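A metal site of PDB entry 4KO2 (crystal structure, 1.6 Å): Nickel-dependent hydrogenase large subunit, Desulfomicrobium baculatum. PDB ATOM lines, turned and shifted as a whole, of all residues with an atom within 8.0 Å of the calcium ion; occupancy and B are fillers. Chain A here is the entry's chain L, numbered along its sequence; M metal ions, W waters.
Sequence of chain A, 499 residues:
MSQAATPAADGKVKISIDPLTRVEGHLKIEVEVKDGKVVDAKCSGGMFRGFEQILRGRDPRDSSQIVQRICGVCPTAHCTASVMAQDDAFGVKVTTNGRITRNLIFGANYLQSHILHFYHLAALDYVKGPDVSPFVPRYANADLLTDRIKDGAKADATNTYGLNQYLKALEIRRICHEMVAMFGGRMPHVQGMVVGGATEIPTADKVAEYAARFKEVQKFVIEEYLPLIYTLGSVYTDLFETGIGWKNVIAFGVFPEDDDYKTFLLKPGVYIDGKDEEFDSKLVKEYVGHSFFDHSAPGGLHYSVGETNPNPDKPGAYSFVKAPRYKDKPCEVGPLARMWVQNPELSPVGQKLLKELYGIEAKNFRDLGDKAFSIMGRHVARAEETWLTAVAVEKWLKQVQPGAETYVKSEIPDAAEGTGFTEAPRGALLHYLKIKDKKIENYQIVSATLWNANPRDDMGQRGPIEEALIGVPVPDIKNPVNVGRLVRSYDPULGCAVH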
ATOM      1  N   PHE A  48     -20.983  -9.996  -6.183  1.00  0.00           N
ATOM      2  CA  PHE A  48     -20.145  -9.386  -7.200  1.00  0.00           C
ATOM      3  C   PHE A  48     -20.631  -9.813  -8.578  1.00  0.00           C
ATOM      4  O   PHE A  48     -20.946 -10.986  -8.788  1.00  0.00           O
ATOM      5  CB  PHE A  48     -18.682  -9.841  -7.003  1.00  0.00           C
ATOM      6  CG  PHE A  48     -17.741  -9.430  -8.115  1.00  0.00           C
ATOM      7  CD1 PHE A  48     -17.225  -8.138  -8.163  1.00  0.00           C
ATOM      8  CD2 PHE A  48     -17.351 -10.341  -9.100  1.00  0.00           C
ATOM      9  CE1 PHE A  48     -16.333  -7.755  -9.175  1.00  0.00           C
ATOM     10  CE2 PHE A  48     -16.471  -9.964 -10.110  1.00  0.00           C
ATOM     11  CZ  PHE A  48     -15.953  -8.659 -10.153  1.00  0.00           C
ATOM     12  N   GLU A  52     -17.030  -3.994 -14.774  1.00  0.00           N
ATOM     13  CA  GLU A  52     -15.830  -3.452 -15.384  1.00  0.00           C
ATOM     14  C   GLU A  52     -15.149  -4.508 -16.276  1.00  0.00           C
ATOM     15  O   GLU A  52     -14.532  -4.160 -17.279  1.00  0.00           O
ATOM     16  CB  GLU A  52     -14.883  -2.917 -14.307  1.00  0.00           C
ATOM     17  CG  GLU A  52     -15.497  -1.741 -13.527  1.00  0.00           C
ATOM     18  CD  GLU A  52     -14.938  -1.579 -12.134  1.00  0.00           C
ATOM     19  OE1 GLU A  52     -14.876  -0.425 -11.642  1.00  0.00           O
ATOM     20  OE2 GLU A  52     -14.562  -2.612 -11.514  1.00  0.00           O
ATOM     21  N   GLU A 286      -8.133   3.883  -4.699  1.00  0.00           N
ATOM     22  CA  GLU A 286      -8.777   2.738  -4.095  1.00  0.00           C
ATOM     23  C   GLU A 286      -7.751   1.741  -3.558  1.00  0.00           C
ATOM     24  O   GLU A 286      -6.814   1.361  -4.253  1.00  0.00           O
ATOM     25  CB  GLU A 286      -9.695   2.053  -5.096  1.00  0.00           C
ATOM     26  CG  GLU A 286     -10.876   2.919  -5.511  1.00  0.00           C
ATOM     27  CD  GLU A 286     -11.766   2.227  -6.506  1.00  0.00           C
ATOM     28  OE1 GLU A 286     -12.843   1.753  -6.100  1.00  0.00           O
ATOM     29  OE2 GLU A 286     -11.353   2.113  -7.685  1.00  0.00           O
ATOM     30  N   PHE A 293      -9.981  -8.518  -4.041  1.00  0.00           N
ATOM     31  CA  PHE A 293      -9.368  -8.104  -5.302  1.00  0.00           C
ATOM     32  C   PHE A 293      -7.854  -8.109  -5.225  1.00  0.00           C
ATOM     33  O   PHE A 293      -7.285  -7.849  -4.160  1.00  0.00           O
ATOM     34  CB  PHE A 293      -9.833  -6.690  -5.704  1.00  0.00           C
ATOM     35  CG  PHE A 293     -11.280  -6.632  -6.038  1.00  0.00           C
ATOM     36  CD1 PHE A 293     -11.742  -7.066  -7.288  1.00  0.00           C
ATOM     37  CD2 PHE A 293     -12.218  -6.210  -5.084  1.00  0.00           C
ATOM     38  CE1 PHE A 293     -13.104  -7.055  -7.581  1.00  0.00           C
ATOM     39  CE2 PHE A 293     -13.564  -6.189  -5.392  1.00  0.00           C
ATOM     40  CZ  PHE A 293     -14.017  -6.620  -6.631  1.00  0.00           C
ATOM     41  N   TYR A 303      -8.237   5.695 -10.089  1.00  0.00           N
ATOM     42  CA  TYR A 303      -9.221   5.004 -10.934  1.00  0.00           C
ATOM     43  C   TYR A 303      -8.822   4.960 -12.418  1.00  0.00           C
ATOM     44  O   TYR A 303      -9.236   4.050 -13.136  1.00  0.00           O
ATOM     45  CB  TYR A 303     -10.617   5.626 -10.774  1.00  0.00           C
ATOM     46  CG  TYR A 303     -10.647   7.091 -11.125  1.00  0.00           C
ATOM     47  CD1 TYR A 303     -10.735   7.502 -12.468  1.00  0.00           C
ATOM     48  CD2 TYR A 303     -10.580   8.062 -10.127  1.00  0.00           C
ATOM     49  CE1 TYR A 303     -10.753   8.865 -12.802  1.00  0.00           C
ATOM     50  CE2 TYR A 303     -10.588   9.423 -10.460  1.00  0.00           C
ATOM     51  CZ  TYR A 303     -10.673   9.815 -11.792  1.00  0.00           C
ATOM     52  OH  TYR A 303     -10.678  11.150 -12.078  1.00  0.00           O
ATOM     53  N   GLY A 306      -7.228   1.843 -12.698  1.00  0.00           N
ATOM     54  CA  GLY A 306      -7.906   0.874 -11.849  1.00  0.00           C
ATOM     55  C   GLY A 306      -7.904  -0.520 -12.452  1.00  0.00           C
ATOM     56  O   GLY A 306      -7.833  -0.682 -13.677  1.00  0.00           O
ATOM     57  N   GLU A 307      -7.983  -1.526 -11.586  1.00  0.00           N
ATOM     58  CA  GLU A 307      -7.906  -2.923 -11.992  1.00  0.00           C
ATOM     59  C   GLU A 307      -9.004  -3.680 -11.290  1.00  0.00           C
ATOM     60  O   GLU A 307      -9.252  -3.461 -10.107  1.00  0.00           O
ATOM     61  CB  GLU A 307      -6.569  -3.520 -11.577  1.00  0.00           C
ATOM     62  CG  GLU A 307      -5.356  -2.944 -12.304  1.00  0.00           C
ATOM     63  CD  GLU A 307      -4.057  -3.400 -11.670  1.00  0.00           C
ATOM     64  OE1 GLU A 307      -4.081  -4.302 -10.785  1.00  0.00           O
ATOM     65  OE2 GLU A 307      -2.998  -2.871 -12.071  1.00  0.00           O
ATOM     66  N   THR A 308      -9.620  -4.602 -12.016  1.00  0.00           N
ATOM     67  CA  THR A 308     -10.702  -5.413 -11.465  1.00  0.00           C
ATOM     68  C   THR A 308     -10.380  -6.891 -11.679  1.00  0.00           C
ATOM     69  O   THR A 308     -10.748  -7.505 -12.697  1.00  0.00           O
ATOM     70  CB  THR A 308     -12.059  -5.013 -12.041  1.00  0.00           C
ATOM     71  OG1 THR A 308     -12.230  -3.607 -11.836  1.00  0.00           O
ATOM     72  CG2 THR A 308     -13.202  -5.749 -11.352  1.00  0.00           C
ATOM     73  N   PHE A 320     -16.542  -7.516  -1.067  1.00  0.00           N
ATOM     74  CA  PHE A 320     -16.369  -7.216  -2.492  1.00  0.00           C
ATOM     75  C   PHE A 320     -16.346  -5.712  -2.793  1.00  0.00           C
ATOM     76  O   PHE A 320     -16.203  -5.317  -3.943  1.00  0.00           O
ATOM     77  CB  PHE A 320     -17.448  -7.878  -3.348  1.00  0.00           C
ATOM     78  CG  PHE A 320     -17.235  -9.355  -3.547  1.00  0.00           C
ATOM     79  CD1 PHE A 320     -16.172  -9.840  -4.316  1.00  0.00           C
ATOM     80  CD2 PHE A 320     -18.117 -10.279  -2.982  1.00  0.00           C
ATOM     81  CE1 PHE A 320     -15.975 -11.212  -4.502  1.00  0.00           C
ATOM     82  CE2 PHE A 320     -17.933 -11.657  -3.166  1.00  0.00           C
ATOM     83  CZ  PHE A 320     -16.859 -12.131  -3.927  1.00  0.00           C
ATOM     84  N   LYS A 322     -14.393  -2.274  -2.757  1.00  0.00           N
ATOM     85  CA  LYS A 322     -13.046  -1.678  -2.622  1.00  0.00           C
ATOM     86  C   LYS A 322     -13.090  -0.549  -1.598  1.00  0.00           C
ATOM     87  O   LYS A 322     -14.166  -0.160  -1.141  1.00  0.00           O
ATOM     88  CB  LYS A 322     -12.525  -1.167  -3.971  1.00  0.00           C
ATOM     89  CG  LYS A 322     -12.373  -2.240  -5.037  1.00  0.00           C
ATOM     90  CD  LYS A 322     -11.633  -1.679  -6.261  1.00  0.00           C
ATOM     91  CE  LYS A 322     -11.429  -2.709  -7.368  1.00  0.00           C
ATOM     92  NZ  LYS A 322     -11.188  -2.055  -8.707  1.00  0.00           N
ATOM     93  N   LEU A 430     -18.291   8.689 -10.318  1.00  0.00           N
ATOM     94  CA  LEU A 430     -17.604   8.899 -11.583  1.00  0.00           C
ATOM     95  C   LEU A 430     -17.496   7.605 -12.364  1.00  0.00           C
ATOM     96  O   LEU A 430     -17.431   6.502 -11.764  1.00  0.00           O
ATOM     97  CB  LEU A 430     -16.227   9.564 -11.402  1.00  0.00           C
ATOM     98  CG  LEU A 430     -15.113   8.788 -10.701  1.00  0.00           C
ATOM     99  CD1 LEU A 430     -14.364   7.871 -11.690  1.00  0.00           C
ATOM    100  CD2 LEU A 430     -14.158   9.770 -10.003  1.00  0.00           C
ATOM    101  N   TYR A 443     -12.738   0.327 -18.180  1.00  0.00           N
ATOM    102  CA  TYR A 443     -13.869   1.123 -17.695  1.00  0.00           C
ATOM    103  C   TYR A 443     -13.839   0.974 -16.185  1.00  0.00           C
ATOM    104  O   TYR A 443     -13.844  -0.149 -15.681  1.00  0.00           O
ATOM    105  CB  TYR A 443     -15.180   0.590 -18.284  1.00  0.00           C
ATOM    106  CG  TYR A 443     -16.336   1.580 -18.244  1.00  0.00           C
ATOM    107  CD1 TYR A 443     -16.996   1.888 -17.045  1.00  0.00           C
ATOM    108  CD2 TYR A 443     -16.788   2.182 -19.417  1.00  0.00           C
ATOM    109  CE1 TYR A 443     -18.066   2.787 -17.033  1.00  0.00           C
ATOM    110  CE2 TYR A 443     -17.829   3.069 -19.407  1.00  0.00           C
ATOM    111  CZ  TYR A 443     -18.475   3.374 -18.228  1.00  0.00           C
ATOM    112  OH  TYR A 443     -19.538   4.255 -18.273  1.00  0.00           O
ATOM    113  N   GLN A 444     -13.783   2.084 -15.470  1.00  0.00           N
ATOM    114  CA  GLN A 444     -13.682   2.031 -14.025  1.00  0.00           C
ATOM    115  C   GLN A 444     -14.776   2.881 -13.396  1.00  0.00           C
ATOM    116  O   GLN A 444     -14.978   4.026 -13.791  1.00  0.00           O
ATOM    117  CB  GLN A 444     -12.294   2.468 -13.528  1.00  0.00           C
ATOM    118  CG  GLN A 444     -11.189   1.443 -13.879  1.00  0.00           C
ATOM    119  CD  GLN A 444     -11.299   0.165 -13.069  1.00  0.00           C
ATOM    120  OE1 GLN A 444     -11.404   0.201 -11.841  1.00  0.00           O
ATOM    121  NE2 GLN A 444     -11.255  -0.977 -13.751  1.00  0.00           N
ATOM    122  N   ILE A 445     -15.497   2.298 -12.451  1.00  0.00           N
ATOM    123  CA  ILE A 445     -16.630   2.940 -11.800  1.00  0.00           C
ATOM    124  C   ILE A 445     -16.276   3.172 -10.345  1.00  0.00           C
ATOM    125  O   ILE A 445     -15.843   2.242  -9.659  1.00  0.00           O
ATOM    126  CB  ILE A 445     -17.877   2.054 -11.928  1.00  0.00           C
ATOM    127  CG1 ILE A 445     -18.268   1.940 -13.411  1.00  0.00           C
ATOM    128  CG2 ILE A 445     -19.024   2.591 -11.091  1.00  0.00           C
ATOM    129  CD1 ILE A 445     -18.873   0.651 -13.796  1.00  0.00           C
ATOM    130  N   VAL A 446     -16.424   4.424  -9.882  1.00  0.00           N
ATOM    131  CA  VAL A 446     -16.210   4.768  -8.471  1.00  0.00           C
ATOM    132  C   VAL A 446     -17.557   5.344  -8.048  1.00  0.00           C
ATOM    133  O   VAL A 446     -17.887   6.476  -8.401  1.00  0.00           O
ATOM    134  CB  VAL A 446     -15.042   5.751  -8.296  1.00  0.00           C
ATOM    135  CG1 VAL A 446     -14.831   6.089  -6.826  1.00  0.00           C
ATOM    136  CG2 VAL A 446     -13.751   5.173  -8.912  1.00  0.00           C
ATOM    137  N   SER A 447     -18.307   4.541  -7.298  1.00  0.00           N
ATOM    138  CA  SER A 447     -19.694   4.852  -7.026  1.00  0.00           C
ATOM    139  C   SER A 447     -19.888   5.400  -5.622  1.00  0.00           C
ATOM    140  O   SER A 447     -18.976   5.422  -4.795  1.00  0.00           O
ATOM    141  CB  SER A 447     -20.544   3.600  -7.201  1.00  0.00           C
ATOM    142  OG  SER A 447     -20.178   2.645  -6.228  1.00  0.00           O
ATOM    143  N   LEU A 450     -19.927   2.913  -2.581  1.00  0.00           N
ATOM    144  CA  LEU A 450     -18.513   2.536  -2.505  1.00  0.00           C
ATOM    145  C   LEU A 450     -17.760   3.382  -1.463  1.00  0.00           C
ATOM    146  O   LEU A 450     -16.965   2.853  -0.683  1.00  0.00           O
ATOM    147  CB  LEU A 450     -17.845   2.685  -3.864  1.00  0.00           C
ATOM    148  CG  LEU A 450     -16.315   2.569  -3.910  1.00  0.00           C
ATOM    149  CD1 LEU A 450     -15.854   1.126  -3.673  1.00  0.00           C
ATOM    150  CD2 LEU A 450     -15.854   3.064  -5.244  1.00  0.00           C
ATOM    151  N   CYS A 496     -24.489  -0.923  -6.469  1.00  0.00           N
ATOM    152  CA  CYS A 496     -23.580   0.154  -6.863  1.00  0.00           C
ATOM    153  C   CYS A 496     -22.221   0.034  -6.235  1.00  0.00           C
ATOM    154  O   CYS A 496     -21.215   0.319  -6.899  1.00  0.00           O
ATOM    155  CB  CYS A 496     -24.136   1.515  -6.484  1.00  0.00           C
ATOM    156  SG  CYS A 496     -25.563   1.994  -7.441  1.00  0.00           S
ATOM    157  N   ALA A 497     -22.179  -0.372  -4.966  1.00  0.00           N
ATOM    158  CA  ALA A 497     -20.895  -0.384  -4.242  1.00  0.00           C
ATOM    159  C   ALA A 497     -19.896  -1.352  -4.875  1.00  0.00           C
ATOM    160  O   ALA A 497     -18.701  -1.061  -4.912  1.00  0.00           O
ATOM    161  CB  ALA A 497     -21.089  -0.750  -2.752  1.00  0.00           C
ATOM    162  N   VAL A 498     -20.411  -2.475  -5.381  1.00  0.00           N
ATOM    163  CA  VAL A 498     -19.553  -3.574  -5.858  1.00  0.00           C
ATOM    164  C   VAL A 498     -19.487  -3.631  -7.382  1.00  0.00           C
ATOM    165  O   VAL A 498     -18.401  -3.829  -7.944  1.00  0.00           O
ATOM    166  CB  VAL A 498     -20.033  -4.957  -5.336  1.00  0.00           C
ATOM    167  CG1 VAL A 498     -19.137  -6.072  -5.915  1.00  0.00           C
ATOM    168  CG2 VAL A 498     -20.048  -4.988  -3.811  1.00  0.00           C
ATOM    169  N   HIS A 499     -20.635  -3.445  -8.026  1.00  0.00           N
ATOM    170  CA  HIS A 499     -20.809  -3.557  -9.483  1.00  0.00           C
ATOM    171  C   HIS A 499     -20.061  -4.768 -10.035  1.00  0.00           C
ATOM    172  O   HIS A 499     -19.296  -4.663 -10.996  1.00  0.00           O
ATOM    173  CB  HIS A 499     -20.467  -2.231 -10.233  1.00  0.00           C
ATOM    174  CG  HIS A 499     -19.242  -1.529  -9.723  1.00  0.00           C
ATOM    175  ND1 HIS A 499     -19.266  -0.724  -8.603  1.00  0.00           N
ATOM    176  CD2 HIS A 499     -17.957  -1.521 -10.162  1.00  0.00           C
ATOM    177  CE1 HIS A 499     -18.054  -0.244  -8.375  1.00  0.00           C
ATOM    178  NE2 HIS A 499     -17.239  -0.718  -9.313  1.00  0.00           N
ATOM    179  OXT HIS A 499     -20.208  -5.879  -9.492  1.00  0.00           O
HETATM  180 CA    CA M   1     -14.916   0.082  -9.344  1.00  0.00          CA
HETATM  181  O   HOH W   1     -14.785   0.307  -7.017  1.00  0.00           O
HETATM  182  O   HOH W   2     -12.747   0.905  -9.522  1.00  0.00           O
HETATM  183  O   HOH W   3     -14.346  -2.050  -8.901  1.00  0.00           O
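Water W3 binds the calcium ion (2.3 Å). The calcium ion is bound by water W2 (2.3 Å). Water W1 binds the calcium ion. OE1 of Glu 52 is bound to the calcium ion (2.4 Å). The calcium ion is bound by the backbone carbonyl oxygen (O) of Ile 445, at 2.4 Å. The calcium ion is bound by NE2 of His 499 (2.5 Å).
Water W2 lies within hydrogen-bond range of OE2 of Glu 286 (2.6 Å), OE1 of Gln 444 (2.8 Å) and NZ of Lys 322 (3.4 Å). Water W3 lies within hydrogen-bond range of OE2 of Glu 52 (2.7 Å) and NZ of Lys 322 (3.2 Å).
Three residues have an atom within 4 Å of the calcium ion: Glu 52, Ile 445 and His 499.
OE2 of Glu 52 is in hydrogen-bond range of OG1 of Thr 308 (2.6 Å). The backbone carbonyl oxygen (O) of Cys 496 is in hydrogen-bond range of a ring nitrogen (ND1) of His 499 (2.8 Å).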
